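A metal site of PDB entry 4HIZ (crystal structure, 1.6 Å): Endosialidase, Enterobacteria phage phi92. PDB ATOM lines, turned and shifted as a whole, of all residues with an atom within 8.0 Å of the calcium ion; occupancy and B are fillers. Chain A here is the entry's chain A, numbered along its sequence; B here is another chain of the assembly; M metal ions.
N of Phe 81 sits at hydrogen-bond distance from OG1 of Thr 79 (3.1 Å). The backbone NH (N) of Asn 83 sits close to the backbone carbonyl oxygen (O) of Ala 515 (3.2 Å). The backbone carbonyl oxygen of Phe 81 sits close to the side-chain amide nitrogen of Asn 83 (3.4 Å). NH2 of Arg 542 of chain B lies close to OD2 of Asp 516, at 3.1 Å. ND2 of Asn 83 sits at hydrogen-bond distance from OD1 of Asp 516 (2.9 Å). OD1 of Asp 516 is in hydrogen-bond range of OG1 of Thr 77 (2.7 Å). N of Gly 490 lies within hydrogen-bond range of O of Asp 516 (3.1 Å). The side-chain carboxylate (OD1) of Asp 78 lies within salt-bridge range of the guanidinium group (NE) of Arg 542 of chain B.
ND2 of Asn 83 touches the calcium ion, at 3.7 Å. Pro 514 touches the calcium ion. Arg 542 of chain B touches the calcium ion (NH2 to CA, 3.5 Å). Of the 23 residues printed, 8 come within 4 Å of the calcium ion.
The calcium ion is bound by the backbone carbonyl oxygen of Thr 79 (2.4 Å), the backbone carbonyl oxygen of His 513 (2.4 Å), the backbone carbonyl oxygen of Ala 515 (2.5 Å), the backbone carbonyl oxygen of Phe 81 (2.5 Å) and the side-chain carboxylate of Asp 516 (2.7 Å). The calcium ion has five donor atoms within binding distance.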
ATOM      1  N   LYS A  75      12.275 -11.287  -6.240  1.00  0.00           N
ATOM      2  CA  LYS A  75      11.589 -10.873  -4.996  1.00  0.00           C
ATOM      3  C   LYS A  75      10.103 -11.173  -5.148  1.00  0.00           C
ATOM      4  O   LYS A  75       9.523 -10.849  -6.194  1.00  0.00           O
ATOM      5  CB  LYS A  75      11.794  -9.356  -4.774  1.00  0.00           C
ATOM      6  CG  LYS A  75      11.233  -8.893  -3.430  1.00  0.00           C
ATOM      7  CD  LYS A  75      11.682  -7.441  -3.139  1.00  0.00           C
ATOM      8  CE  LYS A  75      11.256  -7.051  -1.706  1.00  0.00           C
ATOM      9  NZ  LYS A  75      11.800  -5.671  -1.378  1.00  0.00           N
ATOM     10  N   THR A  77       7.487 -11.096  -2.299  1.00  0.00           N
ATOM     11  CA  THR A  77       6.555 -10.277  -1.544  1.00  0.00           C
ATOM     12  C   THR A  77       7.099  -8.871  -1.415  1.00  0.00           C
ATOM     13  O   THR A  77       8.335  -8.661  -1.475  1.00  0.00           O
ATOM     14  CB  THR A  77       6.225 -10.791  -0.080  1.00  0.00           C
ATOM     15  OG1 THR A  77       7.390 -10.723   0.769  1.00  0.00           O
ATOM     16  CG2 THR A  77       5.756 -12.216  -0.141  1.00  0.00           C
ATOM     17  N   ASP A  78       6.191  -7.926  -1.257  1.00  0.00           N
ATOM     18  CA  ASP A  78       6.626  -6.549  -1.008  1.00  0.00           C
ATOM     19  C   ASP A  78       5.541  -5.842  -0.257  1.00  0.00           C
ATOM     20  O   ASP A  78       4.848  -4.972  -0.790  1.00  0.00           O
ATOM     21  CB  ASP A  78       6.983  -5.858  -2.327  1.00  0.00           C
ATOM     22  CG  ASP A  78       7.644  -4.492  -2.124  1.00  0.00           C
ATOM     23  OD1 ASP A  78       8.088  -4.180  -0.983  1.00  0.00           O
ATOM     24  OD2 ASP A  78       7.738  -3.776  -3.141  1.00  0.00           O
ATOM     25  N   THR A  79       5.420  -6.157   1.048  1.00  0.00           N
ATOM     26  CA  THR A  79       4.407  -5.512   1.880  1.00  0.00           C
ATOM     27  C   THR A  79       5.093  -5.045   3.161  1.00  0.00           C
ATOM     28  O   THR A  79       6.208  -5.487   3.477  1.00  0.00           O
ATOM     29  CB  THR A  79       3.204  -6.470   2.222  1.00  0.00           C
ATOM     30  OG1 THR A  79       3.336  -6.937   3.571  1.00  0.00           O
ATOM     31  CG2 THR A  79       3.092  -7.673   1.256  1.00  0.00           C
ATOM     32  N   PRO A  80       4.442  -4.133   3.903  1.00  0.00           N
ATOM     33  CA  PRO A  80       5.149  -3.562   5.069  1.00  0.00           C
ATOM     34  C   PRO A  80       5.035  -4.445   6.305  1.00  0.00           C
ATOM     35  O   PRO A  80       5.618  -4.108   7.347  1.00  0.00           O
ATOM     36  CB  PRO A  80       4.425  -2.235   5.311  1.00  0.00           C
ATOM     37  CG  PRO A  80       3.015  -2.505   4.829  1.00  0.00           C
ATOM     38  CD  PRO A  80       3.141  -3.484   3.661  1.00  0.00           C
ATOM     39  N   PHE A  81       4.319  -5.549   6.193  1.00  0.00           N
ATOM     40  CA  PHE A  81       4.359  -6.509   7.298  1.00  0.00           C
ATOM     41  C   PHE A  81       5.724  -7.148   7.388  1.00  0.00           C
ATOM     42  O   PHE A  81       6.543  -7.085   6.443  1.00  0.00           O
ATOM     43  CB  PHE A  81       3.297  -7.610   7.097  1.00  0.00           C
ATOM     44  CG  PHE A  81       1.894  -7.130   7.385  1.00  0.00           C
ATOM     45  CD1 PHE A  81       1.382  -7.146   8.685  1.00  0.00           C
ATOM     46  CD2 PHE A  81       1.088  -6.633   6.375  1.00  0.00           C
ATOM     47  CE1 PHE A  81       0.050  -6.708   8.953  1.00  0.00           C
ATOM     48  CE2 PHE A  81      -0.221  -6.189   6.623  1.00  0.00           C
ATOM     49  CZ  PHE A  81      -0.738  -6.226   7.920  1.00  0.00           C
ATOM     50  N   TYR A  82       5.978  -7.771   8.539  1.00  0.00           N
ATOM     51  CA  TYR A  82       7.181  -8.587   8.695  1.00  0.00           C
ATOM     52  C   TYR A  82       6.817  -9.938   8.076  1.00  0.00           C
ATOM     53  O   TYR A  82       6.128 -10.764   8.695  1.00  0.00           O
ATOM     54  CB  TYR A  82       7.532  -8.707  10.205  1.00  0.00           C
ATOM     55  CG  TYR A  82       8.954  -9.176  10.436  1.00  0.00           C
ATOM     56  CD1 TYR A  82       9.332 -10.517  10.229  1.00  0.00           C
ATOM     57  CD2 TYR A  82       9.951  -8.275  10.888  1.00  0.00           C
ATOM     58  CE1 TYR A  82      10.650 -10.935  10.430  1.00  0.00           C
ATOM     59  CE2 TYR A  82      11.257  -8.688  11.068  1.00  0.00           C
ATOM     60  CZ  TYR A  82      11.611 -10.003  10.842  1.00  0.00           C
ATOM     61  OH  TYR A  82      12.921 -10.379  11.047  1.00  0.00           O
ATOM     62  N   ASN A  83       7.231 -10.134   6.819  1.00  0.00           N
ATOM     63  CA  ASN A  83       6.845 -11.315   6.037  1.00  0.00           C
ATOM     64  C   ASN A  83       8.030 -12.251   6.052  1.00  0.00           C
ATOM     65  O   ASN A  83       9.059 -11.961   5.431  1.00  0.00           O
ATOM     66  CB  ASN A  83       6.531 -10.911   4.597  1.00  0.00           C
ATOM     67  CG  ASN A  83       5.375  -9.945   4.526  1.00  0.00           C
ATOM     68  OD1 ASN A  83       4.338 -10.183   5.164  1.00  0.00           O
ATOM     69  ND2 ASN A  83       5.531  -8.849   3.764  1.00  0.00           N
ATOM     70  N   ALA A  84       7.877 -13.413   6.697  1.00  0.00           N
ATOM     71  CA  ALA A  84       9.040 -14.264   6.877  1.00  0.00           C
ATOM     72  C   ALA A  84       8.615 -15.718   7.123  1.00  0.00           C
ATOM     73  O   ALA A  84       7.434 -16.015   7.227  1.00  0.00           O
ATOM     74  CB  ALA A  84       9.892 -13.713   8.087  1.00  0.00           C
ATOM     75  N   GLY A 104       3.483 -10.891   9.942  1.00  0.00           N
ATOM     76  CA  GLY A 104       3.272 -10.354  11.287  1.00  0.00           C
ATOM     77  C   GLY A 104       4.051  -9.065  11.469  1.00  0.00           C
ATOM     78  O   GLY A 104       4.112  -8.221  10.543  1.00  0.00           O
ATOM     79  N   GLY A 490      14.762 -12.369   2.920  1.00  0.00           N
ATOM     80  CA  GLY A 490      15.834 -11.370   2.925  1.00  0.00           C
ATOM     81  C   GLY A 490      15.281 -10.035   3.365  1.00  0.00           C
ATOM     82  O   GLY A 490      14.051  -9.852   3.365  1.00  0.00           O
ATOM     83  N   GLU A 491      16.156  -9.106   3.776  1.00  0.00           N
ATOM     84  CA  GLU A 491      15.702  -7.777   4.188  1.00  0.00           C
ATOM     85  C   GLU A 491      16.150  -6.743   3.184  1.00  0.00           C
ATOM     86  O   GLU A 491      16.487  -7.090   2.029  1.00  0.00           O
ATOM     87  CB  GLU A 491      16.218  -7.437   5.614  1.00  0.00           C
ATOM     88  CG  GLU A 491      15.833  -8.631   6.551  1.00  0.00           C
ATOM     89  CD  GLU A 491      16.196  -8.385   8.020  1.00  0.00           C
ATOM     90  OE1 GLU A 491      16.908  -7.390   8.346  1.00  0.00           O
ATOM     91  OE2 GLU A 491      15.731  -9.207   8.850  1.00  0.00           O
ATOM     92  N   ASP A 492      16.114  -5.486   3.607  1.00  0.00           N
ATOM     93  CA  ASP A 492      16.586  -4.335   2.798  1.00  0.00           C
ATOM     94  C   ASP A 492      17.109  -3.355   3.828  1.00  0.00           C
ATOM     95  O   ASP A 492      16.981  -3.623   5.039  1.00  0.00           O
ATOM     96  CB  ASP A 492      15.472  -3.763   1.856  1.00  0.00           C
ATOM     97  CG  ASP A 492      14.286  -3.129   2.613  1.00  0.00           C
ATOM     98  OD1 ASP A 492      14.476  -2.398   3.592  1.00  0.00           O
ATOM     99  OD2 ASP A 492      13.105  -3.342   2.218  1.00  0.00           O
ATOM    100  N   TRP A 507       3.170  -1.647  11.087  1.00  0.00           N
ATOM    101  CA  TRP A 507       3.625  -1.866   9.726  1.00  0.00           C
ATOM    102  C   TRP A 507       3.345  -0.660   8.839  1.00  0.00           C
ATOM    103  O   TRP A 507       4.067  -0.430   7.887  1.00  0.00           O
ATOM    104  CB  TRP A 507       2.964  -3.145   9.134  1.00  0.00           C
ATOM    105  CG  TRP A 507       1.516  -3.260   9.466  1.00  0.00           C
ATOM    106  CD1 TRP A 507       0.452  -2.705   8.796  1.00  0.00           C
ATOM    107  CD2 TRP A 507       0.952  -3.968  10.575  1.00  0.00           C
ATOM    108  NE1 TRP A 507      -0.744  -3.026   9.436  1.00  0.00           N
ATOM    109  CE2 TRP A 507      -0.445  -3.788  10.530  1.00  0.00           C
ATOM    110  CE3 TRP A 507       1.517  -4.718  11.626  1.00  0.00           C
ATOM    111  CZ2 TRP A 507      -1.306  -4.363  11.477  1.00  0.00           C
ATOM    112  CZ3 TRP A 507       0.662  -5.288  12.552  1.00  0.00           C
ATOM    113  CH2 TRP A 507      -0.736  -5.110  12.482  1.00  0.00           C
ATOM    114  N   ASP A 511       8.420   2.919   6.576  1.00  0.00           N
ATOM    115  CA  ASP A 511       8.582   1.823   5.604  1.00  0.00           C
ATOM    116  C   ASP A 511       8.153   0.465   6.136  1.00  0.00           C
ATOM    117  O   ASP A 511       8.467  -0.580   5.530  1.00  0.00           O
ATOM    118  CB  ASP A 511      10.031   1.768   5.123  1.00  0.00           C
ATOM    119  CG  ASP A 511      10.462   3.114   4.530  1.00  0.00           C
ATOM    120  OD1 ASP A 511       9.850   3.517   3.506  1.00  0.00           O
ATOM    121  OD2 ASP A 511      11.361   3.781   5.100  1.00  0.00           O
ATOM    122  N   GLY A 512       7.498   0.453   7.283  1.00  0.00           N
ATOM    123  CA  GLY A 512       7.152  -0.824   7.907  1.00  0.00           C
ATOM    124  C   GLY A 512       8.397  -1.685   8.097  1.00  0.00           C
ATOM    125  O   GLY A 512       9.487  -1.170   8.407  1.00  0.00           O
ATOM    126  N   HIS A 513       8.236  -3.003   7.944  1.00  0.00           N
ATOM    127  CA  HIS A 513       9.293  -3.971   8.203  1.00  0.00           C
ATOM    128  C   HIS A 513       9.964  -4.445   6.939  1.00  0.00           C
ATOM    129  O   HIS A 513       9.263  -4.719   5.919  1.00  0.00           O
ATOM    130  CB  HIS A 513       8.666  -5.167   8.952  1.00  0.00           C
ATOM    131  CG  HIS A 513       8.055  -4.732  10.236  1.00  0.00           C
ATOM    132  ND1 HIS A 513       8.809  -4.358  11.326  1.00  0.00           N
ATOM    133  CD2 HIS A 513       6.757  -4.509  10.569  1.00  0.00           C
ATOM    134  CE1 HIS A 513       7.998  -3.950  12.295  1.00  0.00           C
ATOM    135  NE2 HIS A 513       6.745  -4.041  11.864  1.00  0.00           N
ATOM    136  N   PRO A 514      11.297  -4.600   6.974  1.00  0.00           N
ATOM    137  CA  PRO A 514      12.048  -4.863   5.730  1.00  0.00           C
ATOM    138  C   PRO A 514      12.044  -6.338   5.354  1.00  0.00           C
ATOM    139  O   PRO A 514      12.582  -6.677   4.295  1.00  0.00           O
ATOM    140  CB  PRO A 514      13.481  -4.427   6.071  1.00  0.00           C
ATOM    141  CG  PRO A 514      13.580  -4.598   7.574  1.00  0.00           C
ATOM    142  CD  PRO A 514      12.190  -4.219   8.089  1.00  0.00           C
ATOM    143  N   ALA A 515      11.505  -7.210   6.208  1.00  0.00           N
ATOM    144  CA  ALA A 515      11.482  -8.638   5.877  1.00  0.00           C
ATOM    145  C   ALA A 515      10.461  -8.964   4.789  1.00  0.00           C
ATOM    146  O   ALA A 515       9.288  -8.633   4.921  1.00  0.00           O
ATOM    147  CB  ALA A 515      11.134  -9.438   7.161  1.00  0.00           C
ATOM    148  N   ASP A 516      10.944  -9.603   3.723  1.00  0.00           N
ATOM    149  CA  ASP A 516      10.105 -10.041   2.589  1.00  0.00           C
ATOM    150  C   ASP A 516      10.710 -11.317   1.997  1.00  0.00           C
ATOM    151  O   ASP A 516      11.794 -11.738   2.401  1.00  0.00           O
ATOM    152  CB  ASP A 516       9.997  -8.910   1.510  1.00  0.00           C
ATOM    153  CG  ASP A 516       8.912  -7.917   1.871  1.00  0.00           C
ATOM    154  OD1 ASP A 516       7.711  -8.293   1.892  1.00  0.00           O
ATOM    155  OD2 ASP A 516       9.261  -6.751   2.171  1.00  0.00           O
ATOM    156  N   LEU A 517      10.002 -11.933   1.044  1.00  0.00           N
ATOM    157  CA  LEU A 517      10.428 -13.238   0.511  1.00  0.00           C
ATOM    158  C   LEU A 517      11.006 -13.130  -0.895  1.00  0.00           C
ATOM    159  O   LEU A 517      10.625 -12.222  -1.662  1.00  0.00           O
ATOM    160  CB  LEU A 517       9.222 -14.216   0.469  1.00  0.00           C
ATOM    161  CG  LEU A 517       8.501 -14.356   1.798  1.00  0.00           C
ATOM    162  CD1 LEU A 517       7.319 -15.324   1.613  1.00  0.00           C
ATOM    163  CD2 LEU A 517       9.446 -14.905   2.900  1.00  0.00           C
ATOM    164  N   ASN B 541       2.916  -3.731  -2.725  1.00  0.00           N
ATOM    165  CA  ASN B 541       1.920  -3.696  -1.656  1.00  0.00           C
ATOM    166  C   ASN B 541       2.357  -2.781  -0.522  1.00  0.00           C
ATOM    167  O   ASN B 541       2.079  -3.033   0.665  1.00  0.00           O
ATOM    168  CB  ASN B 541       1.724  -5.126  -1.135  1.00  0.00           C
ATOM    169  CG  ASN B 541       0.288  -5.560  -1.132  1.00  0.00           C
ATOM    170  OD1 ASN B 541      -0.625  -4.767  -1.325  1.00  0.00           O
ATOM    171  ND2 ASN B 541       0.077  -6.836  -0.867  1.00  0.00           N
ATOM    172  N   ARG B 542       2.995  -1.666  -0.912  1.00  0.00           N
ATOM    173  CA  ARG B 542       3.355  -0.659   0.085  1.00  0.00           C
ATOM    174  C   ARG B 542       2.406   0.525   0.075  1.00  0.00           C
ATOM    175  O   ARG B 542       2.042   1.032   1.125  1.00  0.00           O
ATOM    176  CB  ARG B 542       4.790  -0.135  -0.110  1.00  0.00           C
ATOM    177  CG  ARG B 542       5.920  -1.174  -0.041  1.00  0.00           C
ATOM    178  CD  ARG B 542       5.733  -2.121   1.134  1.00  0.00           C
ATOM    179  NE  ARG B 542       6.925  -2.964   1.309  1.00  0.00           N
ATOM    180  CZ  ARG B 542       7.797  -2.813   2.325  1.00  0.00           C
ATOM    181  NH1 ARG B 542       7.616  -1.846   3.206  1.00  0.00           N
ATOM    182  NH2 ARG B 542       8.821  -3.650   2.465  1.00  0.00           N
HETATM  183 CA    CA M   1       8.129  -6.404   4.580  1.00  0.00          CA
